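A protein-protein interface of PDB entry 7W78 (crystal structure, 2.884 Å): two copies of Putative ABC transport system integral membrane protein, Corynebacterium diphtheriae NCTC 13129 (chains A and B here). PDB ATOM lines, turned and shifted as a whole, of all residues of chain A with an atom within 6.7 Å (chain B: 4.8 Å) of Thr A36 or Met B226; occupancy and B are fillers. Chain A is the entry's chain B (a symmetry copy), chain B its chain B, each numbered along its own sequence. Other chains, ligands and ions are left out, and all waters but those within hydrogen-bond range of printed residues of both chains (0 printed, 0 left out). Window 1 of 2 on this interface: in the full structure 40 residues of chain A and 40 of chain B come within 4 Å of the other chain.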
ATOM      1  N   LEU A  28       2.211 -24.575  17.347  1.00  0.00           N
ATOM      2  CA  LEU A  28       1.804 -25.275  16.132  1.00  0.00           C
ATOM      3  C   LEU A  28       0.471 -24.752  15.621  1.00  0.00           C
ATOM      4  O   LEU A  28       0.303 -24.521  14.419  1.00  0.00           O
ATOM      5  CB  LEU A  28       1.705 -26.778  16.378  1.00  0.00           C
ATOM      6  CG  LEU A  28       1.350 -27.532  15.094  1.00  0.00           C
ATOM      7  CD1 LEU A  28       2.504 -27.459  14.105  1.00  0.00           C
ATOM      8  CD2 LEU A  28       0.959 -28.975  15.363  1.00  0.00           C
ATOM      9  N   MET A  31       0.680 -20.875  14.274  1.00  0.00           N
ATOM     10  CA  MET A  31       1.314 -20.685  12.962  1.00  0.00           C
ATOM     11  C   MET A  31       0.539 -21.381  11.860  1.00  0.00           C
ATOM     12  O   MET A  31       0.293 -20.783  10.797  1.00  0.00           O
ATOM     13  CB  MET A  31       2.773 -21.128  13.021  1.00  0.00           C
ATOM     14  CG  MET A  31       3.408 -20.772  14.357  1.00  0.00           C
ATOM     15  SD  MET A  31       3.360 -19.004  14.713  1.00  0.00           S
ATOM     16  CE  MET A  31       4.309 -18.343  13.412  1.00  0.00           C
ATOM     17  N   LEU A  32       0.100 -22.624  12.091  1.00  0.00           N
ATOM     18  CA  LEU A  32      -0.697 -23.293  11.072  1.00  0.00           C
ATOM     19  C   LEU A  32      -2.010 -22.561  10.828  1.00  0.00           C
ATOM     20  O   LEU A  32      -2.453 -22.447   9.682  1.00  0.00           O
ATOM     21  CB  LEU A  32      -0.944 -24.747  11.437  1.00  0.00           C
ATOM     22  CG  LEU A  32       0.262 -25.642  11.136  1.00  0.00           C
ATOM     23  CD1 LEU A  32      -0.179 -27.061  10.936  1.00  0.00           C
ATOM     24  CD2 LEU A  32       1.039 -25.150   9.916  1.00  0.00           C
ATOM     25  N   THR A  33      -2.619 -22.017  11.883  1.00  0.00           N
ATOM     26  CA  THR A  33      -3.810 -21.195  11.686  1.00  0.00           C
ATOM     27  C   THR A  33      -3.487 -19.972  10.840  1.00  0.00           C
ATOM     28  O   THR A  33      -4.156 -19.703   9.837  1.00  0.00           O
ATOM     29  CB  THR A  33      -4.400 -20.771  13.033  1.00  0.00           C
ATOM     30  OG1 THR A  33      -4.978 -21.911  13.683  1.00  0.00           O
ATOM     31  CG2 THR A  33      -5.470 -19.703  12.844  1.00  0.00           C
ATOM     32  N   GLY A  34      -2.448 -19.227  11.225  1.00  0.00           N
ATOM     33  CA  GLY A  34      -2.096 -18.021  10.495  1.00  0.00           C
ATOM     34  C   GLY A  34      -1.557 -18.284   9.104  1.00  0.00           C
ATOM     35  O   GLY A  34      -1.659 -17.424   8.225  1.00  0.00           O
ATOM     36  N   LEU A  35      -0.971 -19.462   8.883  1.00  0.00           N
ATOM     37  CA  LEU A  35      -0.516 -19.797   7.539  1.00  0.00           C
ATOM     38  C   LEU A  35      -1.681 -20.140   6.620  1.00  0.00           C
ATOM     39  O   LEU A  35      -1.634 -19.823   5.426  1.00  0.00           O
ATOM     40  CB  LEU A  35       0.487 -20.949   7.581  1.00  0.00           C
ATOM     41  CG  LEU A  35       1.911 -20.584   8.005  1.00  0.00           C
ATOM     42  CD1 LEU A  35       2.839 -21.767   7.801  1.00  0.00           C
ATOM     43  CD2 LEU A  35       2.410 -19.369   7.240  1.00  0.00           C
ATOM     44  N   THR A  36      -2.734 -20.776   7.145  1.00  0.00           N
ATOM     45  CA  THR A  36      -3.882 -21.068   6.291  1.00  0.00           C
ATOM     46  C   THR A  36      -4.825 -19.878   6.166  1.00  0.00           C
ATOM     47  O   THR A  36      -5.423 -19.687   5.101  1.00  0.00           O
ATOM     48  CB  THR A  36      -4.657 -22.291   6.790  1.00  0.00           C
ATOM     49  OG1 THR A  36      -5.395 -21.959   7.974  1.00  0.00           O
ATOM     50  CG2 THR A  36      -3.719 -23.449   7.065  1.00  0.00           C
ATOM     51  N   GLN A  37      -4.981 -19.070   7.221  1.00  0.00           N
ATOM     52  CA  GLN A  37      -5.708 -17.815   7.050  1.00  0.00           C
ATOM     53  C   GLN A  37      -5.027 -16.943   6.004  1.00  0.00           C
ATOM     54  O   GLN A  37      -5.696 -16.183   5.295  1.00  0.00           O
ATOM     55  CB  GLN A  37      -5.835 -17.071   8.384  1.00  0.00           C
ATOM     56  CG  GLN A  37      -6.559 -17.865   9.463  1.00  0.00           C
ATOM     57  CD  GLN A  37      -7.299 -16.995  10.478  1.00  0.00           C
ATOM     58  OE1 GLN A  37      -6.902 -15.874  10.755  1.00  0.00           O
ATOM     59  NE2 GLN A  37      -8.370 -17.527  11.041  1.00  0.00           N
ATOM     60  N   GLY A  38      -3.705 -17.065   5.871  1.00  0.00           N
ATOM     61  CA  GLY A  38      -3.013 -16.395   4.782  1.00  0.00           C
ATOM     62  C   GLY A  38      -3.409 -16.940   3.424  1.00  0.00           C
ATOM     63  O   GLY A  38      -3.661 -16.180   2.486  1.00  0.00           O
ATOM     64  N   LEU A  39      -3.468 -18.271   3.298  1.00  0.00           N
ATOM     65  CA  LEU A  39      -3.897 -18.866   2.036  1.00  0.00           C
ATOM     66  C   LEU A  39      -5.321 -18.463   1.683  1.00  0.00           C
ATOM     67  O   LEU A  39      -5.672 -18.392   0.500  1.00  0.00           O
ATOM     68  CB  LEU A  39      -3.778 -20.390   2.089  1.00  0.00           C
ATOM     69  CG  LEU A  39      -2.403 -20.982   1.777  1.00  0.00           C
ATOM     70  CD1 LEU A  39      -2.526 -22.472   1.508  1.00  0.00           C
ATOM     71  CD2 LEU A  39      -1.765 -20.266   0.594  1.00  0.00           C
ATOM     72  N   GLY A  40      -6.153 -18.189   2.689  1.00  0.00           N
ATOM     73  CA  GLY A  40      -7.516 -17.771   2.411  1.00  0.00           C
ATOM     74  C   GLY A  40      -7.587 -16.387   1.796  1.00  0.00           C
ATOM     75  O   GLY A  40      -8.417 -16.127   0.921  1.00  0.00           O
ATOM     76  N   LYS A  41      -6.710 -15.483   2.234  1.00  0.00           N
ATOM     77  CA  LYS A  41      -6.718 -14.111   1.744  1.00  0.00           C
ATOM     78  C   LYS A  41      -6.101 -13.973   0.357  1.00  0.00           C
ATOM     79  O   LYS A  41      -6.129 -12.874  -0.207  1.00  0.00           O
ATOM     80  CB  LYS A  41      -5.994 -13.201   2.741  1.00  0.00           C
ATOM     81  CG  LYS A  41      -6.526 -13.295   4.170  1.00  0.00           C
ATOM     82  CD  LYS A  41      -7.443 -12.131   4.506  1.00  0.00           C
ATOM     83  CE  LYS A  41      -7.496 -11.883   6.006  1.00  0.00           C
ATOM     84  NZ  LYS A  41      -7.218 -10.457   6.332  1.00  0.00           N
ATOM     85  N   LEU A 223      -9.357 -25.727   3.330  1.00  0.00           N
ATOM     86  CA  LEU A 223      -8.817 -24.999   4.475  1.00  0.00           C
ATOM     87  C   LEU A 223      -9.561 -25.329   5.761  1.00  0.00           C
ATOM     88  O   LEU A 223      -8.941 -25.455   6.824  1.00  0.00           O
ATOM     89  CB  LEU A 223      -8.862 -23.497   4.210  1.00  0.00           C
ATOM     90  CG  LEU A 223      -7.980 -23.034   3.056  1.00  0.00           C
ATOM     91  CD1 LEU A 223      -8.422 -21.666   2.580  1.00  0.00           C
ATOM     92  CD2 LEU A 223      -6.529 -23.005   3.497  1.00  0.00           C
ATOM     93  N   MET A 226      -8.288 -28.585   7.142  1.00  0.00           N
ATOM     94  CA  MET A 226      -7.033 -28.463   7.875  1.00  0.00           C
ATOM     95  C   MET A 226      -7.266 -27.912   9.273  1.00  0.00           C
ATOM     96  O   MET A 226      -6.781 -28.470  10.264  1.00  0.00           O
ATOM     97  CB  MET A 226      -6.060 -27.575   7.103  1.00  0.00           C
ATOM     98  CG  MET A 226      -5.472 -28.246   5.885  1.00  0.00           C
ATOM     99  SD  MET A 226      -4.198 -27.249   5.101  1.00  0.00           S
ATOM    100  CE  MET A 226      -5.198 -26.328   3.947  1.00  0.00           C
ATOM    101  N   GLN A 227      -8.012 -26.812   9.375  1.00  0.00           N
ATOM    102  CA  GLN A 227      -8.282 -26.223  10.679  1.00  0.00           C
ATOM    103  C   GLN A 227      -9.148 -27.136  11.546  1.00  0.00           C
ATOM    104  O   GLN A 227      -9.110 -27.022  12.775  1.00  0.00           O
ATOM    105  CB  GLN A 227      -8.900 -24.832  10.476  1.00  0.00           C
ATOM    106  CG  GLN A 227      -9.967 -24.394  11.447  1.00  0.00           C
ATOM    107  CD  GLN A 227     -10.614 -23.083  11.009  1.00  0.00           C
ATOM    108  OE1 GLN A 227      -9.928 -22.111  10.716  1.00  0.00           O
ATOM    109  NE2 GLN A 227     -11.934 -23.066  10.944  1.00  0.00           N
ATOM    110  N   PRO A 301       2.544 -15.397   3.031  1.00  0.00           N
ATOM    111  CA  PRO A 301       1.248 -14.868   3.490  1.00  0.00           C
ATOM    112  C   PRO A 301       0.834 -15.488   4.818  1.00  0.00           C
ATOM    113  O   PRO A 301       0.666 -16.704   4.933  1.00  0.00           O
ATOM    114  CB  PRO A 301       0.285 -15.249   2.356  1.00  0.00           C
ATOM    115  CG  PRO A 301       0.994 -16.310   1.570  1.00  0.00           C
ATOM    116  CD  PRO A 301       2.451 -16.014   1.696  1.00  0.00           C
ATOM    117  N   PHE A 302       0.658 -14.629   5.826  1.00  0.00           N
ATOM    118  CA  PHE A 302       0.395 -15.056   7.205  1.00  0.00           C
ATOM    119  C   PHE A 302      -0.558 -14.044   7.840  1.00  0.00           C
ATOM    120  O   PHE A 302      -0.128 -13.020   8.379  1.00  0.00           O
ATOM    121  CB  PHE A 302       1.697 -15.178   7.989  1.00  0.00           C
ATOM    122  CG  PHE A 302       1.522 -15.677   9.393  1.00  0.00           C
ATOM    123  CD1 PHE A 302       1.249 -14.802  10.429  1.00  0.00           C
ATOM    124  CD2 PHE A 302       1.652 -17.024   9.679  1.00  0.00           C
ATOM    125  CE1 PHE A 302       1.098 -15.263  11.711  1.00  0.00           C
ATOM    126  CE2 PHE A 302       1.503 -17.488  10.963  1.00  0.00           C
ATOM    127  CZ  PHE A 302       1.228 -16.609  11.978  1.00  0.00           C
ATOM    128  N   SER A 303      -1.853 -14.339   7.778  1.00  0.00           N
ATOM    129  CA  SER A 303      -2.879 -13.506   8.390  1.00  0.00           C
ATOM    130  C   SER A 303      -3.230 -14.067   9.761  1.00  0.00           C
ATOM    131  O   SER A 303      -3.418 -15.277   9.909  1.00  0.00           O
ATOM    132  CB  SER A 303      -4.131 -13.444   7.514  1.00  0.00           C
ATOM    133  OG  SER A 303      -5.207 -12.836   8.208  1.00  0.00           O
ATOM    134  N   THR B  36      -2.364 -30.688   2.420  1.00  0.00           N
ATOM    135  CA  THR B  36      -1.601 -29.665   1.711  1.00  0.00           C
ATOM    136  C   THR B  36      -1.009 -30.187   0.408  1.00  0.00           C
ATOM    137  O   THR B  36      -0.911 -29.427  -0.561  1.00  0.00           O
ATOM    138  CB  THR B  36      -0.487 -29.085   2.589  1.00  0.00           C
ATOM    139  OG1 THR B  36       0.576 -30.037   2.730  1.00  0.00           O
ATOM    140  CG2 THR B  36      -1.022 -28.693   3.951  1.00  0.00           C
ATOM    141  N   SER B 222       4.056 -20.905   0.767  1.00  0.00           N
ATOM    142  CA  SER B 222       3.119 -21.058   1.877  1.00  0.00           C
ATOM    143  C   SER B 222       2.952 -22.516   2.292  1.00  0.00           C
ATOM    144  O   SER B 222       2.729 -22.800   3.475  1.00  0.00           O
ATOM    145  CB  SER B 222       1.765 -20.452   1.502  1.00  0.00           C
ATOM    146  OG  SER B 222       1.078 -19.980   2.648  1.00  0.00           O
ATOM    147  N   LEU B 223       3.057 -23.449   1.344  1.00  0.00           N
ATOM    148  CA  LEU B 223       2.876 -24.863   1.665  1.00  0.00           C
ATOM    149  C   LEU B 223       4.104 -25.452   2.345  1.00  0.00           C
ATOM    150  O   LEU B 223       3.974 -26.258   3.274  1.00  0.00           O
ATOM    151  CB  LEU B 223       2.546 -25.650   0.400  1.00  0.00           C
ATOM    152  CG  LEU B 223       1.221 -25.270  -0.251  1.00  0.00           C
ATOM    153  CD1 LEU B 223       1.191 -25.742  -1.689  1.00  0.00           C
ATOM    154  CD2 LEU B 223       0.070 -25.872   0.534  1.00  0.00           C
ATOM    155  N   LEU B 224       5.300 -25.080   1.886  1.00  0.00           N
ATOM    156  CA  LEU B 224       6.510 -25.539   2.555  1.00  0.00           C
ATOM    157  C   LEU B 224       6.566 -25.035   3.990  1.00  0.00           C
ATOM    158  O   LEU B 224       6.991 -25.764   4.894  1.00  0.00           O
ATOM    159  CB  LEU B 224       7.745 -25.091   1.774  1.00  0.00           C
ATOM    160  CG  LEU B 224       8.015 -25.894   0.502  1.00  0.00           C
ATOM    161  CD1 LEU B 224       9.124 -25.261  -0.317  1.00  0.00           C
ATOM    162  CD2 LEU B 224       8.362 -27.332   0.857  1.00  0.00           C
ATOM    163  N   SER B 225       6.132 -23.792   4.218  1.00  0.00           N
ATOM    164  CA  SER B 225       6.095 -23.252   5.574  1.00  0.00           C
ATOM    165  C   SER B 225       5.226 -24.110   6.487  1.00  0.00           C
ATOM    166  O   SER B 225       5.601 -24.388   7.631  1.00  0.00           O
ATOM    167  CB  SER B 225       5.585 -21.812   5.550  1.00  0.00           C
ATOM    168  OG  SER B 225       6.532 -20.939   4.960  1.00  0.00           O
ATOM    169  N   MET B 226       4.067 -24.547   5.993  1.00  0.00           N
ATOM    170  CA  MET B 226       3.190 -25.389   6.799  1.00  0.00           C
ATOM    171  C   MET B 226       3.840 -26.733   7.095  1.00  0.00           C
ATOM    172  O   MET B 226       3.882 -27.176   8.248  1.00  0.00           O
ATOM    173  CB  MET B 226       1.853 -25.584   6.089  1.00  0.00           C
ATOM    174  CG  MET B 226       0.973 -24.358   6.119  1.00  0.00           C
ATOM    175  SD  MET B 226      -0.661 -24.670   5.438  1.00  0.00           S
ATOM    176  CE  MET B 226      -0.365 -24.253   3.729  1.00  0.00           C
ATOM    177  N   GLN B 227       4.357 -27.397   6.062  1.00  0.00           N
ATOM    178  CA  GLN B 227       4.996 -28.689   6.262  1.00  0.00           C
ATOM    179  C   GLN B 227       6.278 -28.566   7.085  1.00  0.00           C
ATOM    180  O   GLN B 227       6.696 -29.547   7.710  1.00  0.00           O
ATOM    181  CB  GLN B 227       5.228 -29.345   4.893  1.00  0.00           C
ATOM    182  CG  GLN B 227       6.488 -30.152   4.710  1.00  0.00           C
ATOM    183  CD  GLN B 227       6.671 -30.578   3.256  1.00  0.00           C
ATOM    184  OE1 GLN B 227       5.763 -31.127   2.645  1.00  0.00           O
ATOM    185  NE2 GLN B 227       7.838 -30.305   2.700  1.00  0.00           N
ATOM    186  N   ALA B 228       6.869 -27.371   7.144  1.00  0.00           N
ATOM    187  CA  ALA B 228       8.033 -27.141   7.997  1.00  0.00           C
ATOM    188  C   ALA B 228       7.633 -27.012   9.466  1.00  0.00           C
ATOM    189  O   ALA B 228       8.139 -27.744  10.324  1.00  0.00           O
ATOM    190  CB  ALA B 228       8.792 -25.893   7.538  1.00  0.00           C
ATOM    191  N   PHE B 229       6.729 -26.077   9.775  1.00  0.00           N
ATOM    192  CA  PHE B 229       6.298 -25.904  11.157  1.00  0.00           C
ATOM    193  C   PHE B 229       5.669 -27.170  11.705  1.00  0.00           C
ATOM    194  O   PHE B 229       5.855 -27.505  12.881  1.00  0.00           O
ATOM    195  CB  PHE B 229       5.317 -24.741  11.269  1.00  0.00           C
ATOM    196  CG  PHE B 229       5.977 -23.413  11.306  1.00  0.00           C
ATOM    197  CD1 PHE B 229       7.241 -23.280  11.855  1.00  0.00           C
ATOM    198  CD2 PHE B 229       5.356 -22.300  10.777  1.00  0.00           C
ATOM    199  CE1 PHE B 229       7.865 -22.061  11.889  1.00  0.00           C
ATOM    200  CE2 PHE B 229       5.979 -21.075  10.808  1.00  0.00           C
ATOM    201  CZ  PHE B 229       7.235 -20.956  11.364  1.00  0.00           C
ATOM    202  N   LEU B 230       4.928 -27.896  10.872  1.00  0.00           N
ATOM    203  CA  LEU B 230       4.270 -29.100  11.362  1.00  0.00           C
ATOM    204  C   LEU B 230       5.293 -30.134  11.810  1.00  0.00           C
ATOM    205  O   LEU B 230       5.173 -30.700  12.900  1.00  0.00           O
ATOM    206  CB  LEU B 230       3.337 -29.669  10.299  1.00  0.00           C
ATOM    207  CG  LEU B 230       2.880 -31.097  10.618  1.00  0.00           C
ATOM    208  CD1 LEU B 230       1.831 -31.098  11.733  1.00  0.00           C
ATOM    209  CD2 LEU B 230       2.321 -31.754   9.365  1.00  0.00           C
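O of Leu A32 sits close to OG1 of Thr A36.
The side-chain hydroxyl (OG1) of Thr A36 is in hydrogen-bond range of the backbone carbonyl oxygen (O) of Thr A33.
Among the printed residues, pairs that only touch across the chains: Leu A28 with Phe B229 (3.6 Å), Leu A28 with Leu B230 (3.7 Å), Met A31 with Phe B229 (3.6 Å), Leu A32 with Met B226 (3.8 Å), Leu A35 with Ser B222 (3.9 Å), Leu A35 with Ser B225 (3.6 Å), Leu A35 with Met B226 (3.5 Å), Leu A35 with Phe B229 (3.9 Å), Thr A36 with Met B226 (3.7 Å), Leu A39 with Ser B222 (3.5 Å), Leu A39 with Met B226 (3.6 Å), Met A226 with Thr B36 (3.7 Å) and Pro A301 with Ser B222 (3.8 Å).
Thr A36 touches just one residue of chain B: Met B226.
Met B226 touches just these residues of chain A: Leu A32 (3.8 Å), Leu A35 (3.5 Å), Thr A36 (3.7 Å) and Leu A39 (3.6 Å).
Of the printed residues of chain B, Leu A35 touches Ser B222 (3.9 Å), Ser B225 (3.6 Å), Met B226 (3.5 Å) and Phe B229 (3.9 Å).
Printed residues of chain B within 4 Å of Leu A39: Ser B222 (3.5 Å) and Met B226 (3.6 Å).
Of the printed residues of chain B, Leu A32 touches Met B226.
Of the printed residues of chain B, Pro A301 touches Ser B222.
Of the printed residues of chain A, Ser B222 touches Leu A35, Leu A39 and Pro A301.
Thr A33 touches none of the printed residues of chain B.
Leu A223 touches none of the printed residues of chain B.
The nearest printed residue of chain B that does not touch Thr A36 is Ser B222 (5.9 Å).
The nearest residue of chain A that does not touch Met B226 is Met A226 (4.4 Å).
The nearest printed residue of chain B that does not touch Pro A301 is Ser B225 (7.1 Å).
Hydrophobic or aromatic side chains of chain A within 4 Å of the printed part of chain B: Leu A28, Met A31, Leu A32, Leu A35, Leu A39, Met A226 and Pro A301.
Printed residues of chain B that touch a printed residue of chain A: Thr B36, Ser B222, Ser B225, Met B226, Phe B229 and Leu B230.
Hydrophobic or aromatic side chains of chain B within 4 Å of the printed part of chain A: Met B226 and Phe B229.
Among the printed residues, no Asp or Glu carboxylate lies within 4 Å of a Lys or Arg side-chain nitrogen of the other chain.
Thr A36 touches Met B226, and with the chains exchanged Met A226 touches Thr B36.
Positions printed for both chains: 36, 223, 226 and 227.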
